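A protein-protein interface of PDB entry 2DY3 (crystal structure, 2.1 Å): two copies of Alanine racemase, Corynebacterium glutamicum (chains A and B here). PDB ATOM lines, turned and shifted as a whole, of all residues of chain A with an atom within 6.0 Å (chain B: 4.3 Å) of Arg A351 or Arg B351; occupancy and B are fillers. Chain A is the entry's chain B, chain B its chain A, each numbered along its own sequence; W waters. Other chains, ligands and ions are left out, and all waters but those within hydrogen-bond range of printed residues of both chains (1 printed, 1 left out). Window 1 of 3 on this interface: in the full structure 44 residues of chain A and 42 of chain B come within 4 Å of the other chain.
The guanidinium group of Arg A351 sits at hydrogen-bond distance from the backbone carbonyl oxygen of Tyr B275 (3.0 Å). The guanidinium group (NE) of Arg A351 lies close to the guanidinium group (NH2) of Arg B351 (3.4 Å).
The side-chain sulfur of Cys A350 sits at hydrogen-bond distance from the backbone carbonyl oxygen of Tyr A346 (3.5 Å). The guanidinium group (NH1) of Arg A351 sits at hydrogen-bond distance from the backbone carbonyl oxygen (O) of Glu A347, 2.5 Å away.
Among the printed residues, pairs that only touch across the chains: Tyr A346 with Tyr B275 (3.2 Å), Glu A347 with Tyr B275 (3.4 Å) and Tyr A275 with Glu B347 (3.6 Å).
Of the printed residues of chain B, Glu A347 touches Tyr B275 (3.4 Å). Of the printed residues of chain B, Arg A351 touches Tyr B275 and Arg B351. Printed residues of chain A within 4 Å of Tyr B275: Tyr A346, Glu A347 and Arg A351. Arg B351 touches just one residue of chain A: Arg A351. The nearest printed residue of chain B that does not touch Tyr A275 is Arg B351 (4.4 Å).
Printed residues of chain A that touch a printed residue of chain B: Tyr A275, Tyr A346, Glu A347 and Arg A351. Hydrophobic or aromatic side chains of chain B within 4 Å of the printed part of chain A: Tyr B275.
Tyr A275 touches Glu B347, and with the chains exchanged Glu A347 touches Tyr B275. Arg A351 touches Tyr B275, but with the chains exchanged Tyr A275 does not touch Arg B351 (4.4 Å). Arg A351 touches its own counterpart, Arg B351. 10 positions are printed for both chains.
Water W1 bridges the guanidinium group (NE) of Arg A351 (2.7 Å) and the guanidinium group (NH2) of Arg B351 (2.9 Å).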
ATOM      1  N   ASN A  39      -5.557 -11.746  16.014  1.00  0.00           N
ATOM      2  CA  ASN A  39      -5.698 -11.033  14.745  1.00  0.00           C
ATOM      3  C   ASN A  39      -4.682  -9.905  14.545  1.00  0.00           C
ATOM      4  O   ASN A  39      -4.793  -9.143  13.589  1.00  0.00           O
ATOM      5  CB  ASN A  39      -7.119 -10.466  14.629  1.00  0.00           C
ATOM      6  CG  ASN A  39      -7.520 -10.156  13.192  1.00  0.00           C
ATOM      7  OD1 ASN A  39      -8.408  -9.338  12.948  1.00  0.00           O
ATOM      8  ND2 ASN A  39      -6.879 -10.820  12.242  1.00  0.00           N
ATOM      9  N   TRP A 238      -8.423  -0.044  13.217  1.00  0.00           N
ATOM     10  CA  TRP A 238      -9.033  -0.495  11.963  1.00  0.00           C
ATOM     11  C   TRP A 238      -9.520   0.773  11.271  1.00  0.00           C
ATOM     12  O   TRP A 238     -10.330   1.515  11.827  1.00  0.00           O
ATOM     13  CB  TRP A 238     -10.209  -1.445  12.254  1.00  0.00           C
ATOM     14  CG  TRP A 238     -10.723  -2.223  11.056  1.00  0.00           C
ATOM     15  CD1 TRP A 238     -10.020  -2.559   9.932  1.00  0.00           C
ATOM     16  CD2 TRP A 238     -12.016  -2.831  10.914  1.00  0.00           C
ATOM     17  NE1 TRP A 238     -10.791  -3.337   9.107  1.00  0.00           N
ATOM     18  CE2 TRP A 238     -12.018  -3.523   9.684  1.00  0.00           C
ATOM     19  CE3 TRP A 238     -13.168  -2.863  11.709  1.00  0.00           C
ATOM     20  CZ2 TRP A 238     -13.129  -4.241   9.229  1.00  0.00           C
ATOM     21  CZ3 TRP A 238     -14.270  -3.575  11.256  1.00  0.00           C
ATOM     22  CH2 TRP A 238     -14.242  -4.255  10.028  1.00  0.00           C
ATOM     23  N   TYR A 275     -19.445  -6.670   5.143  1.00  0.00           N
ATOM     24  CA  TYR A 275     -19.442  -7.867   5.984  1.00  0.00           C
ATOM     25  C   TYR A 275     -18.432  -8.916   5.550  1.00  0.00           C
ATOM     26  O   TYR A 275     -18.084  -9.805   6.328  1.00  0.00           O
ATOM     27  CB  TYR A 275     -20.842  -8.495   6.116  1.00  0.00           C
ATOM     28  CG  TYR A 275     -21.586  -8.792   4.834  1.00  0.00           C
ATOM     29  CD1 TYR A 275     -22.489  -7.880   4.303  1.00  0.00           C
ATOM     30  CD2 TYR A 275     -21.400  -9.996   4.166  1.00  0.00           C
ATOM     31  CE1 TYR A 275     -23.189  -8.162   3.142  1.00  0.00           C
ATOM     32  CE2 TYR A 275     -22.087 -10.286   3.004  1.00  0.00           C
ATOM     33  CZ  TYR A 275     -22.984  -9.366   2.498  1.00  0.00           C
ATOM     34  OH  TYR A 275     -23.692  -9.662   1.360  1.00  0.00           O
ATOM     35  N   ASP A 277     -15.553  -8.193   5.041  1.00  0.00           N
ATOM     36  CA  ASP A 277     -14.313  -7.723   5.646  1.00  0.00           C
ATOM     37  C   ASP A 277     -14.348  -7.731   7.174  1.00  0.00           C
ATOM     38  O   ASP A 277     -13.379  -7.353   7.824  1.00  0.00           O
ATOM     39  CB  ASP A 277     -13.988  -6.315   5.122  1.00  0.00           C
ATOM     40  CG  ASP A 277     -13.951  -6.255   3.598  1.00  0.00           C
ATOM     41  OD1 ASP A 277     -13.014  -6.831   2.996  1.00  0.00           O
ATOM     42  OD2 ASP A 277     -14.869  -5.640   3.002  1.00  0.00           O
ATOM     43  N   GLY A 278     -15.465  -8.159   7.746  1.00  0.00           N
ATOM     44  CA  GLY A 278     -15.561  -8.207   9.193  1.00  0.00           C
ATOM     45  C   GLY A 278     -16.603  -7.289   9.800  1.00  0.00           C
ATOM     46  O   GLY A 278     -16.890  -7.381  10.993  1.00  0.00           O
ATOM     47  N   MET A 279     -17.155  -6.388   8.997  1.00  0.00           N
ATOM     48  CA  MET A 279     -18.171  -5.472   9.490  1.00  0.00           C
ATOM     49  C   MET A 279     -19.511  -6.184   9.502  1.00  0.00           C
ATOM     50  O   MET A 279     -20.123  -6.391   8.454  1.00  0.00           O
ATOM     51  CB  MET A 279     -18.280  -4.238   8.597  1.00  0.00           C
ATOM     52  CG  MET A 279     -19.336  -3.239   9.059  1.00  0.00           C
ATOM     53  SD  MET A 279     -18.886  -2.326  10.576  1.00  0.00           S
ATOM     54  CE  MET A 279     -19.446  -3.374  11.799  1.00  0.00           C
ATOM     55  N   PRO A 280     -19.981  -6.574  10.691  1.00  0.00           N
ATOM     56  CA  PRO A 280     -21.262  -7.270  10.847  1.00  0.00           C
ATOM     57  C   PRO A 280     -22.424  -6.458  10.280  1.00  0.00           C
ATOM     58  O   PRO A 280     -22.444  -5.225  10.381  1.00  0.00           O
ATOM     59  CB  PRO A 280     -21.383  -7.431  12.360  1.00  0.00           C
ATOM     60  CG  PRO A 280     -19.962  -7.511  12.809  1.00  0.00           C
ATOM     61  CD  PRO A 280     -19.299  -6.436  11.988  1.00  0.00           C
ATOM     62  N   PHE A 327     -12.301   1.894  14.541  1.00  0.00           N
ATOM     63  CA  PHE A 327     -11.946   1.771  15.951  1.00  0.00           C
ATOM     64  C   PHE A 327     -10.429   1.774  16.072  1.00  0.00           C
ATOM     65  O   PHE A 327      -9.723   1.272  15.199  1.00  0.00           O
ATOM     66  CB  PHE A 327     -12.572   0.518  16.600  1.00  0.00           C
ATOM     67  CG  PHE A 327     -11.882  -0.785  16.272  1.00  0.00           C
ATOM     68  CD1 PHE A 327     -10.684  -1.127  16.874  1.00  0.00           C
ATOM     69  CD2 PHE A 327     -12.473  -1.695  15.411  1.00  0.00           C
ATOM     70  CE1 PHE A 327     -10.093  -2.356  16.627  1.00  0.00           C
ATOM     71  CE2 PHE A 327     -11.886  -2.927  15.160  1.00  0.00           C
ATOM     72  CZ  PHE A 327     -10.696  -3.256  15.771  1.00  0.00           C
ATOM     73  N   TYR A 346     -12.693  -8.569  22.776  1.00  0.00           N
ATOM     74  CA  TYR A 346     -12.020  -9.761  22.252  1.00  0.00           C
ATOM     75  C   TYR A 346     -12.505 -10.023  20.825  1.00  0.00           C
ATOM     76  O   TYR A 346     -11.714 -10.306  19.920  1.00  0.00           O
ATOM     77  CB  TYR A 346     -12.365 -11.005  23.076  1.00  0.00           C
ATOM     78  CG  TYR A 346     -11.787 -11.081  24.473  1.00  0.00           C
ATOM     79  CD1 TYR A 346     -12.391 -10.426  25.535  1.00  0.00           C
ATOM     80  CD2 TYR A 346     -10.671 -11.873  24.738  1.00  0.00           C
ATOM     81  CE1 TYR A 346     -11.910 -10.562  26.822  1.00  0.00           C
ATOM     82  CE2 TYR A 346     -10.181 -12.015  26.023  1.00  0.00           C
ATOM     83  CZ  TYR A 346     -10.806 -11.357  27.064  1.00  0.00           C
ATOM     84  OH  TYR A 346     -10.345 -11.513  28.351  1.00  0.00           O
ATOM     85  N   GLU A 347     -13.818  -9.936  20.633  1.00  0.00           N
ATOM     86  CA  GLU A 347     -14.406 -10.200  19.326  1.00  0.00           C
ATOM     87  C   GLU A 347     -14.153  -9.108  18.293  1.00  0.00           C
ATOM     88  O   GLU A 347     -13.904  -9.403  17.125  1.00  0.00           O
ATOM     89  CB  GLU A 347     -15.912 -10.459  19.457  1.00  0.00           C
ATOM     90  CG  GLU A 347     -16.580 -10.828  18.127  1.00  0.00           C
ATOM     91  CD  GLU A 347     -17.997 -11.370  18.295  1.00  0.00           C
ATOM     92  OE1 GLU A 347     -18.818 -10.706  18.956  1.00  0.00           O
ATOM     93  OE2 GLU A 347     -18.292 -12.460  17.761  1.00  0.00           O
ATOM     94  N   VAL A 348     -14.198  -7.848  18.711  1.00  0.00           N
ATOM     95  CA  VAL A 348     -13.970  -6.767  17.764  1.00  0.00           C
ATOM     96  C   VAL A 348     -12.563  -6.796  17.149  1.00  0.00           C
ATOM     97  O   VAL A 348     -12.415  -6.573  15.951  1.00  0.00           O
ATOM     98  CB  VAL A 348     -14.240  -5.382  18.410  1.00  0.00           C
ATOM     99  CG1 VAL A 348     -15.685  -5.319  18.916  1.00  0.00           C
ATOM    100  CG2 VAL A 348     -13.278  -5.126  19.533  1.00  0.00           C
ATOM    101  N   VAL A 349     -11.527  -7.080  17.938  1.00  0.00           N
ATOM    102  CA  VAL A 349     -10.188  -7.111  17.353  1.00  0.00           C
ATOM    103  C   VAL A 349     -10.009  -8.291  16.401  1.00  0.00           C
ATOM    104  O   VAL A 349      -9.150  -8.260  15.521  1.00  0.00           O
ATOM    105  CB  VAL A 349      -9.079  -7.152  18.427  1.00  0.00           C
ATOM    106  CG1 VAL A 349      -9.147  -5.879  19.280  1.00  0.00           C
ATOM    107  CG2 VAL A 349      -9.209  -8.408  19.281  1.00  0.00           C
ATOM    108  N   CYS A 350     -10.833  -9.321  16.571  1.00  0.00           N
ATOM    109  CA  CYS A 350     -10.772 -10.503  15.713  1.00  0.00           C
ATOM    110  C   CYS A 350     -11.598 -10.322  14.446  1.00  0.00           C
ATOM    111  O   CYS A 350     -11.502 -11.132  13.524  1.00  0.00           O
ATOM    112  CB  CYS A 350     -11.296 -11.743  16.455  1.00  0.00           C
ATOM    113  SG  CYS A 350     -10.141 -12.505  17.620  1.00  0.00           S
ATOM    114  N   ARG A 351     -12.404  -9.264  14.391  1.00  0.00           N
ATOM    115  CA  ARG A 351     -13.267  -9.031  13.236  1.00  0.00           C
ATOM    116  C   ARG A 351     -12.649  -8.619  11.899  1.00  0.00           C
ATOM    117  O   ARG A 351     -13.027  -9.163  10.857  1.00  0.00           O
ATOM    118  CB  ARG A 351     -14.367  -8.028  13.599  1.00  0.00           C
ATOM    119  CG  ARG A 351     -15.415  -8.572  14.565  1.00  0.00           C
ATOM    120  CD  ARG A 351     -16.223  -9.721  13.952  1.00  0.00           C
ATOM    121  NE  ARG A 351     -15.378 -10.839  13.535  1.00  0.00           N
ATOM    122  CZ  ARG A 351     -14.649 -11.586  14.361  1.00  0.00           C
ATOM    123  NH1 ARG A 351     -14.659 -11.343  15.665  1.00  0.00           N
ATOM    124  NH2 ARG A 351     -13.891 -12.567  13.879  1.00  0.00           N
ATOM    125  N   PRO A 352     -11.709  -7.654  11.900  1.00  0.00           N
ATOM    126  CA  PRO A 352     -11.068  -7.192  10.657  1.00  0.00           C
ATOM    127  C   PRO A 352     -10.510  -8.332   9.812  1.00  0.00           C
ATOM    128  O   PRO A 352      -9.560  -9.002  10.209  1.00  0.00           O
ATOM    129  CB  PRO A 352      -9.981  -6.242  11.164  1.00  0.00           C
ATOM    130  CG  PRO A 352     -10.633  -5.641  12.383  1.00  0.00           C
ATOM    131  CD  PRO A 352     -11.206  -6.892  13.054  1.00  0.00           C
ATOM    132  N   THR A 353     -11.099  -8.531   8.636  1.00  0.00           N
ATOM    133  CA  THR A 353     -10.696  -9.617   7.749  1.00  0.00           C
ATOM    134  C   THR A 353     -10.927  -9.250   6.271  1.00  0.00           C
ATOM    135  O   THR A 353     -11.009  -8.074   5.921  1.00  0.00           O
ATOM    136  CB  THR A 353     -11.496 -10.904   8.127  1.00  0.00           C
ATOM    137  OG1 THR A 353     -10.966 -12.040   7.439  1.00  0.00           O
ATOM    138  CG2 THR A 353     -12.974 -10.742   7.776  1.00  0.00           C
ATOM    139  N   GLY A 354     -11.005 -10.258   5.406  1.00  0.00           N
ATOM    140  CA  GLY A 354     -11.241 -10.013   3.990  1.00  0.00           C
ATOM    141  C   GLY A 354     -10.202  -9.167   3.278  1.00  0.00           C
ATOM    142  O   GLY A 354      -9.030  -9.540   3.206  1.00  0.00           O
ATOM    143  N   TYR B 275     -15.443 -17.524  17.934  1.00  0.00           N
ATOM    144  CA  TYR B 275     -15.661 -16.284  17.199  1.00  0.00           C
ATOM    145  C   TYR B 275     -14.424 -15.777  16.454  1.00  0.00           C
ATOM    146  O   TYR B 275     -14.510 -14.836  15.670  1.00  0.00           O
ATOM    147  CB  TYR B 275     -16.224 -15.189  18.120  1.00  0.00           C
ATOM    148  CG  TYR B 275     -15.426 -14.908  19.368  1.00  0.00           C
ATOM    149  CD1 TYR B 275     -15.828 -15.405  20.607  1.00  0.00           C
ATOM    150  CD2 TYR B 275     -14.278 -14.135  19.313  1.00  0.00           C
ATOM    151  CE1 TYR B 275     -15.105 -15.133  21.752  1.00  0.00           C
ATOM    152  CE2 TYR B 275     -13.551 -13.861  20.447  1.00  0.00           C
ATOM    153  CZ  TYR B 275     -13.964 -14.358  21.662  1.00  0.00           C
ATOM    154  OH  TYR B 275     -13.229 -14.070  22.784  1.00  0.00           O
ATOM    155  N   ASP B 277     -12.936 -17.740  14.558  1.00  0.00           N
ATOM    156  CA  ASP B 277     -13.016 -18.596  13.386  1.00  0.00           C
ATOM    157  C   ASP B 277     -14.273 -18.342  12.557  1.00  0.00           C
ATOM    158  O   ASP B 277     -14.502 -19.009  11.551  1.00  0.00           O
ATOM    159  CB  ASP B 277     -12.984 -20.061  13.821  1.00  0.00           C
ATOM    160  CG  ASP B 277     -11.758 -20.393  14.647  1.00  0.00           C
ATOM    161  OD1 ASP B 277     -10.628 -20.250  14.121  1.00  0.00           O
ATOM    162  OD2 ASP B 277     -11.933 -20.795  15.821  1.00  0.00           O
ATOM    163  N   GLY B 278     -15.103 -17.400  12.988  1.00  0.00           N
ATOM    164  CA  GLY B 278     -16.294 -17.114  12.218  1.00  0.00           C
ATOM    165  C   GLY B 278     -17.611 -17.390  12.913  1.00  0.00           C
ATOM    166  O   GLY B 278     -18.665 -17.055  12.373  1.00  0.00           O
ATOM    167  N   GLU B 347     -23.446 -13.675   3.750  1.00  0.00           N
ATOM    168  CA  GLU B 347     -22.557 -13.498   4.887  1.00  0.00           C
ATOM    169  C   GLU B 347     -22.040 -14.795   5.479  1.00  0.00           C
ATOM    170  O   GLU B 347     -20.868 -14.866   5.863  1.00  0.00           O
ATOM    171  CB  GLU B 347     -23.261 -12.675   5.975  1.00  0.00           C
ATOM    172  CG  GLU B 347     -22.437 -12.430   7.236  1.00  0.00           C
ATOM    173  CD  GLU B 347     -23.070 -11.388   8.148  1.00  0.00           C
ATOM    174  OE1 GLU B 347     -24.296 -11.461   8.372  1.00  0.00           O
ATOM    175  OE2 GLU B 347     -22.349 -10.501   8.645  1.00  0.00           O
ATOM    176  N   VAL B 348     -22.890 -15.823   5.554  1.00  0.00           N
ATOM    177  CA  VAL B 348     -22.441 -17.081   6.139  1.00  0.00           C
ATOM    178  C   VAL B 348     -21.315 -17.719   5.346  1.00  0.00           C
ATOM    179  O   VAL B 348     -20.365 -18.218   5.938  1.00  0.00           O
ATOM    180  CB  VAL B 348     -23.594 -18.123   6.316  1.00  0.00           C
ATOM    181  CG1 VAL B 348     -24.649 -17.578   7.272  1.00  0.00           C
ATOM    182  CG2 VAL B 348     -24.205 -18.471   4.992  1.00  0.00           C
ATOM    183  N   VAL B 349     -21.381 -17.706   4.016  1.00  0.00           N
ATOM    184  CA  VAL B 349     -20.283 -18.325   3.275  1.00  0.00           C
ATOM    185  C   VAL B 349     -18.995 -17.520   3.422  1.00  0.00           C
ATOM    186  O   VAL B 349     -17.908 -18.041   3.177  1.00  0.00           O
ATOM    187  CB  VAL B 349     -20.606 -18.551   1.766  1.00  0.00           C
ATOM    188  CG1 VAL B 349     -21.713 -19.595   1.631  1.00  0.00           C
ATOM    189  CG2 VAL B 349     -20.990 -17.244   1.083  1.00  0.00           C
ATOM    190  N   CYS B 350     -19.116 -16.261   3.839  1.00  0.00           N
ATOM    191  CA  CYS B 350     -17.941 -15.418   4.059  1.00  0.00           C
ATOM    192  C   CYS B 350     -17.399 -15.570   5.472  1.00  0.00           C
ATOM    193  O   CYS B 350     -16.282 -15.139   5.753  1.00  0.00           O
ATOM    194  CB  CYS B 350     -18.268 -13.933   3.853  1.00  0.00           C
ATOM    195  SG  CYS B 350     -18.497 -13.385   2.152  1.00  0.00           S
ATOM    196  N   ARG B 351     -18.174 -16.181   6.365  1.00  0.00           N
ATOM    197  CA  ARG B 351     -17.745 -16.313   7.757  1.00  0.00           C
ATOM    198  C   ARG B 351     -16.619 -17.277   8.119  1.00  0.00           C
ATOM    199  O   ARG B 351     -15.763 -16.934   8.917  1.00  0.00           O
ATOM    200  CB  ARG B 351     -18.952 -16.589   8.659  1.00  0.00           C
ATOM    201  CG  ARG B 351     -19.831 -15.370   8.855  1.00  0.00           C
ATOM    202  CD  ARG B 351     -18.981 -14.115   9.075  1.00  0.00           C
ATOM    203  NE  ARG B 351     -18.121 -14.208  10.255  1.00  0.00           N
ATOM    204  CZ  ARG B 351     -17.166 -13.332  10.555  1.00  0.00           C
ATOM    205  NH1 ARG B 351     -16.942 -12.292   9.760  1.00  0.00           N
ATOM    206  NH2 ARG B 351     -16.429 -13.494  11.646  1.00  0.00           N
ATOM    207  N   PRO B 352     -16.615 -18.497   7.562  1.00  0.00           N
ATOM    208  CA  PRO B 352     -15.538 -19.435   7.899  1.00  0.00           C
ATOM    209  C   PRO B 352     -14.166 -18.803   7.687  1.00  0.00           C
ATOM    210  O   PRO B 352     -13.794 -18.462   6.564  1.00  0.00           O
ATOM    211  CB  PRO B 352     -15.796 -20.607   6.957  1.00  0.00           C
ATOM    212  CG  PRO B 352     -17.299 -20.605   6.841  1.00  0.00           C
ATOM    213  CD  PRO B 352     -17.602 -19.126   6.668  1.00  0.00           C
ATOM    214  N   THR B 353     -13.417 -18.658   8.776  1.00  0.00           N
ATOM    215  CA  THR B 353     -12.098 -18.041   8.721  1.00  0.00           C
ATOM    216  C   THR B 353     -11.230 -18.546   9.878  1.00  0.00           C
ATOM    217  O   THR B 353     -11.478 -19.612  10.429  1.00  0.00           O
ATOM    218  CB  THR B 353     -12.242 -16.498   8.802  1.00  0.00           C
ATOM    219  OG1 THR B 353     -10.956 -15.878   8.698  1.00  0.00           O
ATOM    220  CG2 THR B 353     -12.887 -16.094  10.116  1.00  0.00           C
HETATM  221  O   HOH W   1     -14.236 -11.598  11.203  1.00  0.00           O
